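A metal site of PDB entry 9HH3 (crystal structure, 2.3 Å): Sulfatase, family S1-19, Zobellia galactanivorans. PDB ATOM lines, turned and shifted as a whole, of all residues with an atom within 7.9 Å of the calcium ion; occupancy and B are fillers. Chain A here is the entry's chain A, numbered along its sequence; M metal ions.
The side-chain carboxylate of Asp 25 lies within salt-bridge range of the guanidinium group of Arg 69 (3.7 Å).
The side-chain hydroxyl (OG) of Ser 282 sits at hydrogen-bond distance from the backbone carbonyl oxygen (O) of Asn 284 (2.8 Å).
The side-chain amino group (NZ) of Lys 124 is in salt-bridge range of the side-chain carboxylate (OD2) of Asp 25 (2.8 Å).
N of Asp 283 is in hydrogen-bond range of O of Cys 24.
NH2 of Arg 69 sits close to OD2 of Asp 283 (3.0 Å).
The backbone NH of His 225 lies within hydrogen-bond range of the backbone carbonyl oxygen of Asp 25.
OD2 of Asp 26 is in salt-bridge range of NZ of Lys 301, 2.8 Å away.
OG of Ser 68 is in hydrogen-bond range of O of Asp 283 (2.7 Å).
Five residues have an atom within 4 Å of the calcium ion: Asp 25, Asp 26, DDZ 65, Asp 283 and Asn 284.
Along chain A the residues within 4 Å of the calcium ion span positions 25 to 284.
The nearest printed residue that does not touch the calcium ion is Lys 301 (4.1 Å).
The calcium ion is bound by OD1 of Asp 25, OD1 of Asp 26, OD2 of Asp 283, OD1 of Asn 284, OD1 of Asp 283 and OG1 of DDZ 65.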
ATOM      1  N   LEU A  23     -28.424 -20.445   0.476  1.00  0.00           N
ATOM      2  CA  LEU A  23     -27.423 -21.227   1.181  1.00  0.00           C
ATOM      3  C   LEU A  23     -27.465 -20.809   2.636  1.00  0.00           C
ATOM      4  O   LEU A  23     -27.193 -19.639   2.962  1.00  0.00           O
ATOM      5  CB  LEU A  23     -26.033 -21.004   0.601  1.00  0.00           C
ATOM      6  CG  LEU A  23     -24.910 -21.870   1.187  1.00  0.00           C
ATOM      7  CD1 LEU A  23     -25.115 -23.385   0.858  1.00  0.00           C
ATOM      8  CD2 LEU A  23     -23.532 -21.357   0.713  1.00  0.00           C
ATOM      9  N   CYS A  24     -27.885 -21.725   3.495  1.00  0.00           N
ATOM     10  CA  CYS A  24     -27.791 -21.510   4.920  1.00  0.00           C
ATOM     11  C   CYS A  24     -26.434 -22.010   5.412  1.00  0.00           C
ATOM     12  O   CYS A  24     -25.696 -22.706   4.695  1.00  0.00           O
ATOM     13  CB  CYS A  24     -28.927 -22.202   5.655  1.00  0.00           C
ATOM     14  SG  CYS A  24     -30.411 -21.206   5.628  1.00  0.00           S
ATOM     15  N   ASP A  25     -26.115 -21.640   6.638  1.00  0.00           N
ATOM     16  CA  ASP A  25     -24.798 -21.885   7.230  1.00  0.00           C
ATOM     17  C   ASP A  25     -24.962 -22.730   8.483  1.00  0.00           C
ATOM     18  O   ASP A  25     -25.528 -22.268   9.473  1.00  0.00           O
ATOM     19  CB  ASP A  25     -24.137 -20.546   7.535  1.00  0.00           C
ATOM     20  CG  ASP A  25     -22.678 -20.669   7.874  1.00  0.00           C
ATOM     21  OD1 ASP A  25     -22.135 -21.813   7.954  1.00  0.00           O
ATOM     22  OD2 ASP A  25     -22.062 -19.596   8.108  1.00  0.00           O
ATOM     23  N   ASP A  26     -24.479 -23.988   8.444  1.00  0.00           N
ATOM     24  CA  ASP A  26     -24.550 -24.890   9.591  1.00  0.00           C
ATOM     25  C   ASP A  26     -25.986 -25.328   9.941  1.00  0.00           C
ATOM     26  O   ASP A  26     -26.301 -25.597  11.111  1.00  0.00           O
ATOM     27  CB  ASP A  26     -23.916 -24.252  10.840  1.00  0.00           C
ATOM     28  CG  ASP A  26     -22.419 -24.057  10.710  1.00  0.00           C
ATOM     29  OD1 ASP A  26     -21.840 -24.416   9.656  1.00  0.00           O
ATOM     30  OD2 ASP A  26     -21.830 -23.533  11.686  1.00  0.00           O
ATOM     31  N   LEU A  27     -26.871 -25.430   8.952  1.00  0.00           N
ATOM     32  CA  LEU A  27     -28.232 -25.895   9.239  1.00  0.00           C
ATOM     33  C   LEU A  27     -28.246 -27.412   9.438  1.00  0.00           C
ATOM     34  O   LEU A  27     -27.725 -28.152   8.606  1.00  0.00           O
ATOM     35  CB  LEU A  27     -29.162 -25.481   8.076  1.00  0.00           C
ATOM     36  CG  LEU A  27     -30.612 -25.935   8.152  1.00  0.00           C
ATOM     37  CD1 LEU A  27     -31.441 -25.093   9.113  1.00  0.00           C
ATOM     38  CD2 LEU A  27     -31.224 -25.928   6.780  1.00  0.00           C
ATOM     39  N   HIS A  62     -17.523 -30.829   1.377  1.00  0.00           N
ATOM     40  CA  HIS A  62     -16.608 -30.805   2.511  1.00  0.00           C
ATOM     41  C   HIS A  62     -17.430 -30.568   3.770  1.00  0.00           C
ATOM     42  O   HIS A  62     -18.411 -29.808   3.700  1.00  0.00           O
ATOM     43  CB  HIS A  62     -15.514 -29.734   2.378  1.00  0.00           C
ATOM     44  CG  HIS A  62     -14.329 -29.947   3.271  1.00  0.00           C
ATOM     45  ND1 HIS A  62     -13.364 -30.903   3.011  1.00  0.00           N
ATOM     46  CD2 HIS A  62     -13.936 -29.320   4.402  1.00  0.00           C
ATOM     47  CE1 HIS A  62     -12.453 -30.876   3.969  1.00  0.00           C
ATOM     48  NE2 HIS A  62     -12.771 -29.920   4.818  1.00  0.00           N
ATOM     49  N   PRO A  63     -17.078 -31.178   4.909  1.00  0.00           N
ATOM     50  CA  PRO A  63     -17.938 -31.045   6.083  1.00  0.00           C
ATOM     51  C   PRO A  63     -17.787 -29.743   6.868  1.00  0.00           C
ATOM     52  O   PRO A  63     -18.324 -29.694   7.967  1.00  0.00           O
ATOM     53  CB  PRO A  63     -17.567 -32.270   6.945  1.00  0.00           C
ATOM     54  CG  PRO A  63     -16.128 -32.544   6.577  1.00  0.00           C
ATOM     55  CD  PRO A  63     -16.046 -32.226   5.086  1.00  0.00           C
ATOM     56  N   PHE A  64     -17.150 -28.686   6.339  1.00  0.00           N
ATOM     57  CA  PHE A  64     -17.268 -27.377   6.979  1.00  0.00           C
ATOM     58  C   PHE A  64     -17.090 -26.218   5.981  1.00  0.00           C
ATOM     59  O   PHE A  64     -16.627 -26.396   4.861  1.00  0.00           O
ATOM     60  CB  PHE A  64     -16.302 -27.226   8.178  1.00  0.00           C
ATOM     61  CG  PHE A  64     -14.832 -27.421   7.871  1.00  0.00           C
ATOM     62  CD1 PHE A  64     -14.096 -26.419   7.257  1.00  0.00           C
ATOM     63  CD2 PHE A  64     -14.149 -28.559   8.327  1.00  0.00           C
ATOM     64  CE1 PHE A  64     -12.722 -26.574   7.031  1.00  0.00           C
ATOM     65  CE2 PHE A  64     -12.773 -28.724   8.111  1.00  0.00           C
ATOM     66  CZ  PHE A  64     -12.054 -27.726   7.447  1.00  0.00           C
ATOM     67  N   DDZ A  65     -17.452 -25.025   6.480  1.00  0.00           N
ATOM     68  CA  DDZ A  65     -17.684 -23.684   5.842  1.00  0.00           C
ATOM     69  C   DDZ A  65     -16.848 -23.401   4.580  1.00  0.00           C
ATOM     70  O   DDZ A  65     -17.424 -23.436   3.469  1.00  0.00           O
ATOM     71  OG1 DDZ A  65     -18.335 -22.655   7.990  1.00  0.00           O
ATOM     72  OG2 DDZ A  65     -17.275 -21.297   6.390  1.00  0.00           O
ATOM     73  CB  DDZ A  65     -17.403 -22.615   6.920  1.00  0.00           C
ATOM     74  N   GLY A  66     -15.586 -23.023   4.722  1.00  0.00           N
ATOM     75  CA  GLY A  66     -14.778 -22.481   3.640  1.00  0.00           C
ATOM     76  C   GLY A  66     -14.578 -23.380   2.442  1.00  0.00           C
ATOM     77  O   GLY A  66     -14.766 -22.958   1.292  1.00  0.00           O
ATOM     78  N   SER A  68     -16.251 -26.089   1.606  1.00  0.00           N
ATOM     79  CA  SER A  68     -17.538 -26.383   0.981  1.00  0.00           C
ATOM     80  C   SER A  68     -17.933 -25.242   0.052  1.00  0.00           C
ATOM     81  O   SER A  68     -18.325 -25.482  -1.101  1.00  0.00           O
ATOM     82  CB  SER A  68     -18.593 -26.595   2.040  1.00  0.00           C
ATOM     83  OG  SER A  68     -19.854 -26.671   1.431  1.00  0.00           O
ATOM     84  N   ARG A  69     -17.803 -24.006   0.524  1.00  0.00           N
ATOM     85  CA  ARG A  69     -18.184 -22.869  -0.301  1.00  0.00           C
ATOM     86  C   ARG A  69     -17.256 -22.712  -1.497  1.00  0.00           C
ATOM     87  O   ARG A  69     -17.734 -22.536  -2.623  1.00  0.00           O
ATOM     88  CB  ARG A  69     -18.196 -21.602   0.544  1.00  0.00           C
ATOM     89  CG  ARG A  69     -19.372 -21.556   1.473  1.00  0.00           C
ATOM     90  CD  ARG A  69     -19.135 -20.607   2.624  1.00  0.00           C
ATOM     91  NE  ARG A  69     -20.143 -20.850   3.642  1.00  0.00           N
ATOM     92  CZ  ARG A  69     -21.363 -20.324   3.645  1.00  0.00           C
ATOM     93  NH1 ARG A  69     -21.714 -19.417   2.758  1.00  0.00           N
ATOM     94  NH2 ARG A  69     -22.247 -20.741   4.546  1.00  0.00           N
ATOM     95  N   ASN A  86     -10.048 -23.848   6.367  1.00  0.00           N
ATOM     96  CA  ASN A  86     -10.666 -22.530   6.494  1.00  0.00           C
ATOM     97  C   ASN A  86      -9.603 -21.438   6.478  1.00  0.00           C
ATOM     98  O   ASN A  86      -8.502 -21.616   6.993  1.00  0.00           O
ATOM     99  CB  ASN A  86     -11.420 -22.386   7.816  1.00  0.00           C
ATOM    100  CG  ASN A  86     -12.852 -22.821   7.726  1.00  0.00           C
ATOM    101  OD1 ASN A  86     -13.398 -23.021   6.638  1.00  0.00           O
ATOM    102  ND2 ASN A  86     -13.499 -22.945   8.881  1.00  0.00           N
ATOM    103  N   LYS A 124     -22.624 -13.975   3.469  1.00  0.00           N
ATOM    104  CA  LYS A 124     -21.294 -14.441   3.820  1.00  0.00           C
ATOM    105  C   LYS A 124     -20.458 -14.770   2.579  1.00  0.00           C
ATOM    106  O   LYS A 124     -20.969 -15.329   1.601  1.00  0.00           O
ATOM    107  CB  LYS A 124     -21.420 -15.685   4.704  1.00  0.00           C
ATOM    108  CG  LYS A 124     -20.194 -16.572   4.795  1.00  0.00           C
ATOM    109  CD  LYS A 124     -20.415 -17.629   5.853  1.00  0.00           C
ATOM    110  CE  LYS A 124     -19.228 -18.583   5.967  1.00  0.00           C
ATOM    111  NZ  LYS A 124     -19.433 -19.370   7.196  1.00  0.00           N
ATOM    112  N   HIS A 126     -16.173 -15.445   2.672  1.00  0.00           N
ATOM    113  CA  HIS A 126     -15.186 -16.366   3.245  1.00  0.00           C
ATOM    114  C   HIS A 126     -14.316 -17.069   2.191  1.00  0.00           C
ATOM    115  O   HIS A 126     -13.780 -18.171   2.435  1.00  0.00           O
ATOM    116  CB  HIS A 126     -15.833 -17.403   4.156  1.00  0.00           C
ATOM    117  CG  HIS A 126     -14.920 -17.935   5.217  1.00  0.00           C
ATOM    118  ND1 HIS A 126     -15.219 -19.044   5.970  1.00  0.00           N
ATOM    119  CD2 HIS A 126     -13.735 -17.480   5.672  1.00  0.00           C
ATOM    120  CE1 HIS A 126     -14.240 -19.261   6.834  1.00  0.00           C
ATOM    121  NE2 HIS A 126     -13.329 -18.327   6.677  1.00  0.00           N
ATOM    122  N   GLY A 149     -15.892 -15.188   7.699  1.00  0.00           N
ATOM    123  CA  GLY A 149     -16.601 -16.427   7.944  1.00  0.00           C
ATOM    124  C   GLY A 149     -17.847 -16.336   8.792  1.00  0.00           C
ATOM    125  O   GLY A 149     -18.603 -17.308   8.848  1.00  0.00           O
ATOM    126  N   TYR A 221     -26.941 -16.591   3.491  1.00  0.00           N
ATOM    127  CA  TYR A 221     -27.276 -16.305   4.881  1.00  0.00           C
ATOM    128  C   TYR A 221     -26.211 -16.869   5.817  1.00  0.00           C
ATOM    129  O   TYR A 221     -25.736 -17.991   5.632  1.00  0.00           O
ATOM    130  CB  TYR A 221     -28.618 -16.938   5.248  1.00  0.00           C
ATOM    131  CG  TYR A 221     -29.855 -16.320   4.635  1.00  0.00           C
ATOM    132  CD1 TYR A 221     -30.353 -15.098   5.092  1.00  0.00           C
ATOM    133  CD2 TYR A 221     -30.555 -16.989   3.641  1.00  0.00           C
ATOM    134  CE1 TYR A 221     -31.501 -14.557   4.554  1.00  0.00           C
ATOM    135  CE2 TYR A 221     -31.714 -16.453   3.110  1.00  0.00           C
ATOM    136  CZ  TYR A 221     -32.193 -15.241   3.564  1.00  0.00           C
ATOM    137  OH  TYR A 221     -33.353 -14.726   3.032  1.00  0.00           O
ATOM    138  N   ASN A 222     -25.869 -16.119   6.849  1.00  0.00           N
ATOM    139  CA  ASN A 222     -25.024 -16.757   7.861  1.00  0.00           C
ATOM    140  C   ASN A 222     -25.825 -17.499   8.916  1.00  0.00           C
ATOM    141  O   ASN A 222     -25.259 -18.379   9.571  1.00  0.00           O
ATOM    142  CB  ASN A 222     -24.077 -15.741   8.518  1.00  0.00           C
ATOM    143  CG  ASN A 222     -24.807 -14.633   9.238  1.00  0.00           C
ATOM    144  OD1 ASN A 222     -25.799 -14.072   8.744  1.00  0.00           O
ATOM    145  ND2 ASN A 222     -24.311 -14.297  10.421  1.00  0.00           N
ATOM    146  N   HIS A 225     -25.658 -20.099  11.914  1.00  0.00           N
ATOM    147  CA  HIS A 225     -24.303 -20.136  12.461  1.00  0.00           C
ATOM    148  C   HIS A 225     -24.176 -19.250  13.704  1.00  0.00           C
ATOM    149  O   HIS A 225     -24.865 -18.233  13.842  1.00  0.00           O
ATOM    150  CB  HIS A 225     -23.361 -19.672  11.353  1.00  0.00           C
ATOM    151  CG  HIS A 225     -21.914 -19.858  11.591  1.00  0.00           C
ATOM    152  ND1 HIS A 225     -21.214 -19.107  12.505  1.00  0.00           N
ATOM    153  CD2 HIS A 225     -21.007 -20.623  10.950  1.00  0.00           C
ATOM    154  CE1 HIS A 225     -19.938 -19.457  12.451  1.00  0.00           C
ATOM    155  NE2 HIS A 225     -19.789 -20.370  11.511  1.00  0.00           N
ATOM    156  N   SER A 282     -27.876 -26.363   2.770  1.00  0.00           N
ATOM    157  CA  SER A 282     -26.935 -25.942   3.788  1.00  0.00           C
ATOM    158  C   SER A 282     -25.514 -26.167   3.311  1.00  0.00           C
ATOM    159  O   SER A 282     -25.244 -27.060   2.495  1.00  0.00           O
ATOM    160  CB  SER A 282     -27.169 -26.700   5.081  1.00  0.00           C
ATOM    161  OG  SER A 282     -26.265 -26.271   6.066  1.00  0.00           O
ATOM    162  N   ASP A 283     -24.584 -25.361   3.818  1.00  0.00           N
ATOM    163  CA  ASP A 283     -23.214 -25.539   3.349  1.00  0.00           C
ATOM    164  C   ASP A 283     -22.502 -26.720   4.008  1.00  0.00           C
ATOM    165  O   ASP A 283     -21.476 -27.172   3.487  1.00  0.00           O
ATOM    166  CB  ASP A 283     -22.377 -24.286   3.581  1.00  0.00           C
ATOM    167  CG  ASP A 283     -22.108 -24.029   5.039  1.00  0.00           C
ATOM    168  OD1 ASP A 283     -22.913 -24.431   5.916  1.00  0.00           O
ATOM    169  OD2 ASP A 283     -21.069 -23.396   5.310  1.00  0.00           O
ATOM    170  N   ASN A 284     -23.032 -27.234   5.116  1.00  0.00           N
ATOM    171  CA  ASN A 284     -22.494 -28.427   5.772  1.00  0.00           C
ATOM    172  C   ASN A 284     -23.469 -28.847   6.859  1.00  0.00           C
ATOM    173  O   ASN A 284     -24.533 -28.238   7.030  1.00  0.00           O
ATOM    174  CB  ASN A 284     -21.075 -28.204   6.348  1.00  0.00           C
ATOM    175  CG  ASN A 284     -20.978 -26.974   7.244  1.00  0.00           C
ATOM    176  OD1 ASN A 284     -20.322 -25.990   6.911  1.00  0.00           O
ATOM    177  ND2 ASN A 284     -21.623 -27.022   8.394  1.00  0.00           N
ATOM    178  N   GLY A 285     -23.133 -29.915   7.562  1.00  0.00           N
ATOM    179  CA  GLY A 285     -24.008 -30.424   8.611  1.00  0.00           C
ATOM    180  C   GLY A 285     -24.125 -29.476   9.799  1.00  0.00           C
ATOM    181  O   GLY A 285     -23.331 -28.550   9.991  1.00  0.00           O
ATOM    182  N   GLY A 286     -25.165 -29.689  10.603  1.00  0.00           N
ATOM    183  CA  GLY A 286     -25.366 -28.874  11.779  1.00  0.00           C
ATOM    184  C   GLY A 286     -24.343 -29.171  12.856  1.00  0.00           C
ATOM    185  O   GLY A 286     -23.891 -30.303  13.009  1.00  0.00           O
ATOM    186  N   LYS A 301     -21.219 -31.242  12.367  1.00  0.00           N
ATOM    187  CA  LYS A 301     -20.379 -30.442  11.482  1.00  0.00           C
ATOM    188  C   LYS A 301     -18.912 -30.817  11.631  1.00  0.00           C
ATOM    189  O   LYS A 301     -18.388 -30.927  12.742  1.00  0.00           O
ATOM    190  CB  LYS A 301     -20.567 -28.964  11.812  1.00  0.00           C
ATOM    191  CG  LYS A 301     -19.470 -28.050  11.222  1.00  0.00           C
ATOM    192  CD  LYS A 301     -19.759 -26.597  11.539  1.00  0.00           C
ATOM    193  CE  LYS A 301     -18.705 -25.647  10.974  1.00  0.00           C
ATOM    194  NZ  LYS A 301     -19.116 -24.264  11.240  1.00  0.00           N
HETATM  195 CA    CA M   1     -20.997 -23.710   7.655  1.00  0.00          CA
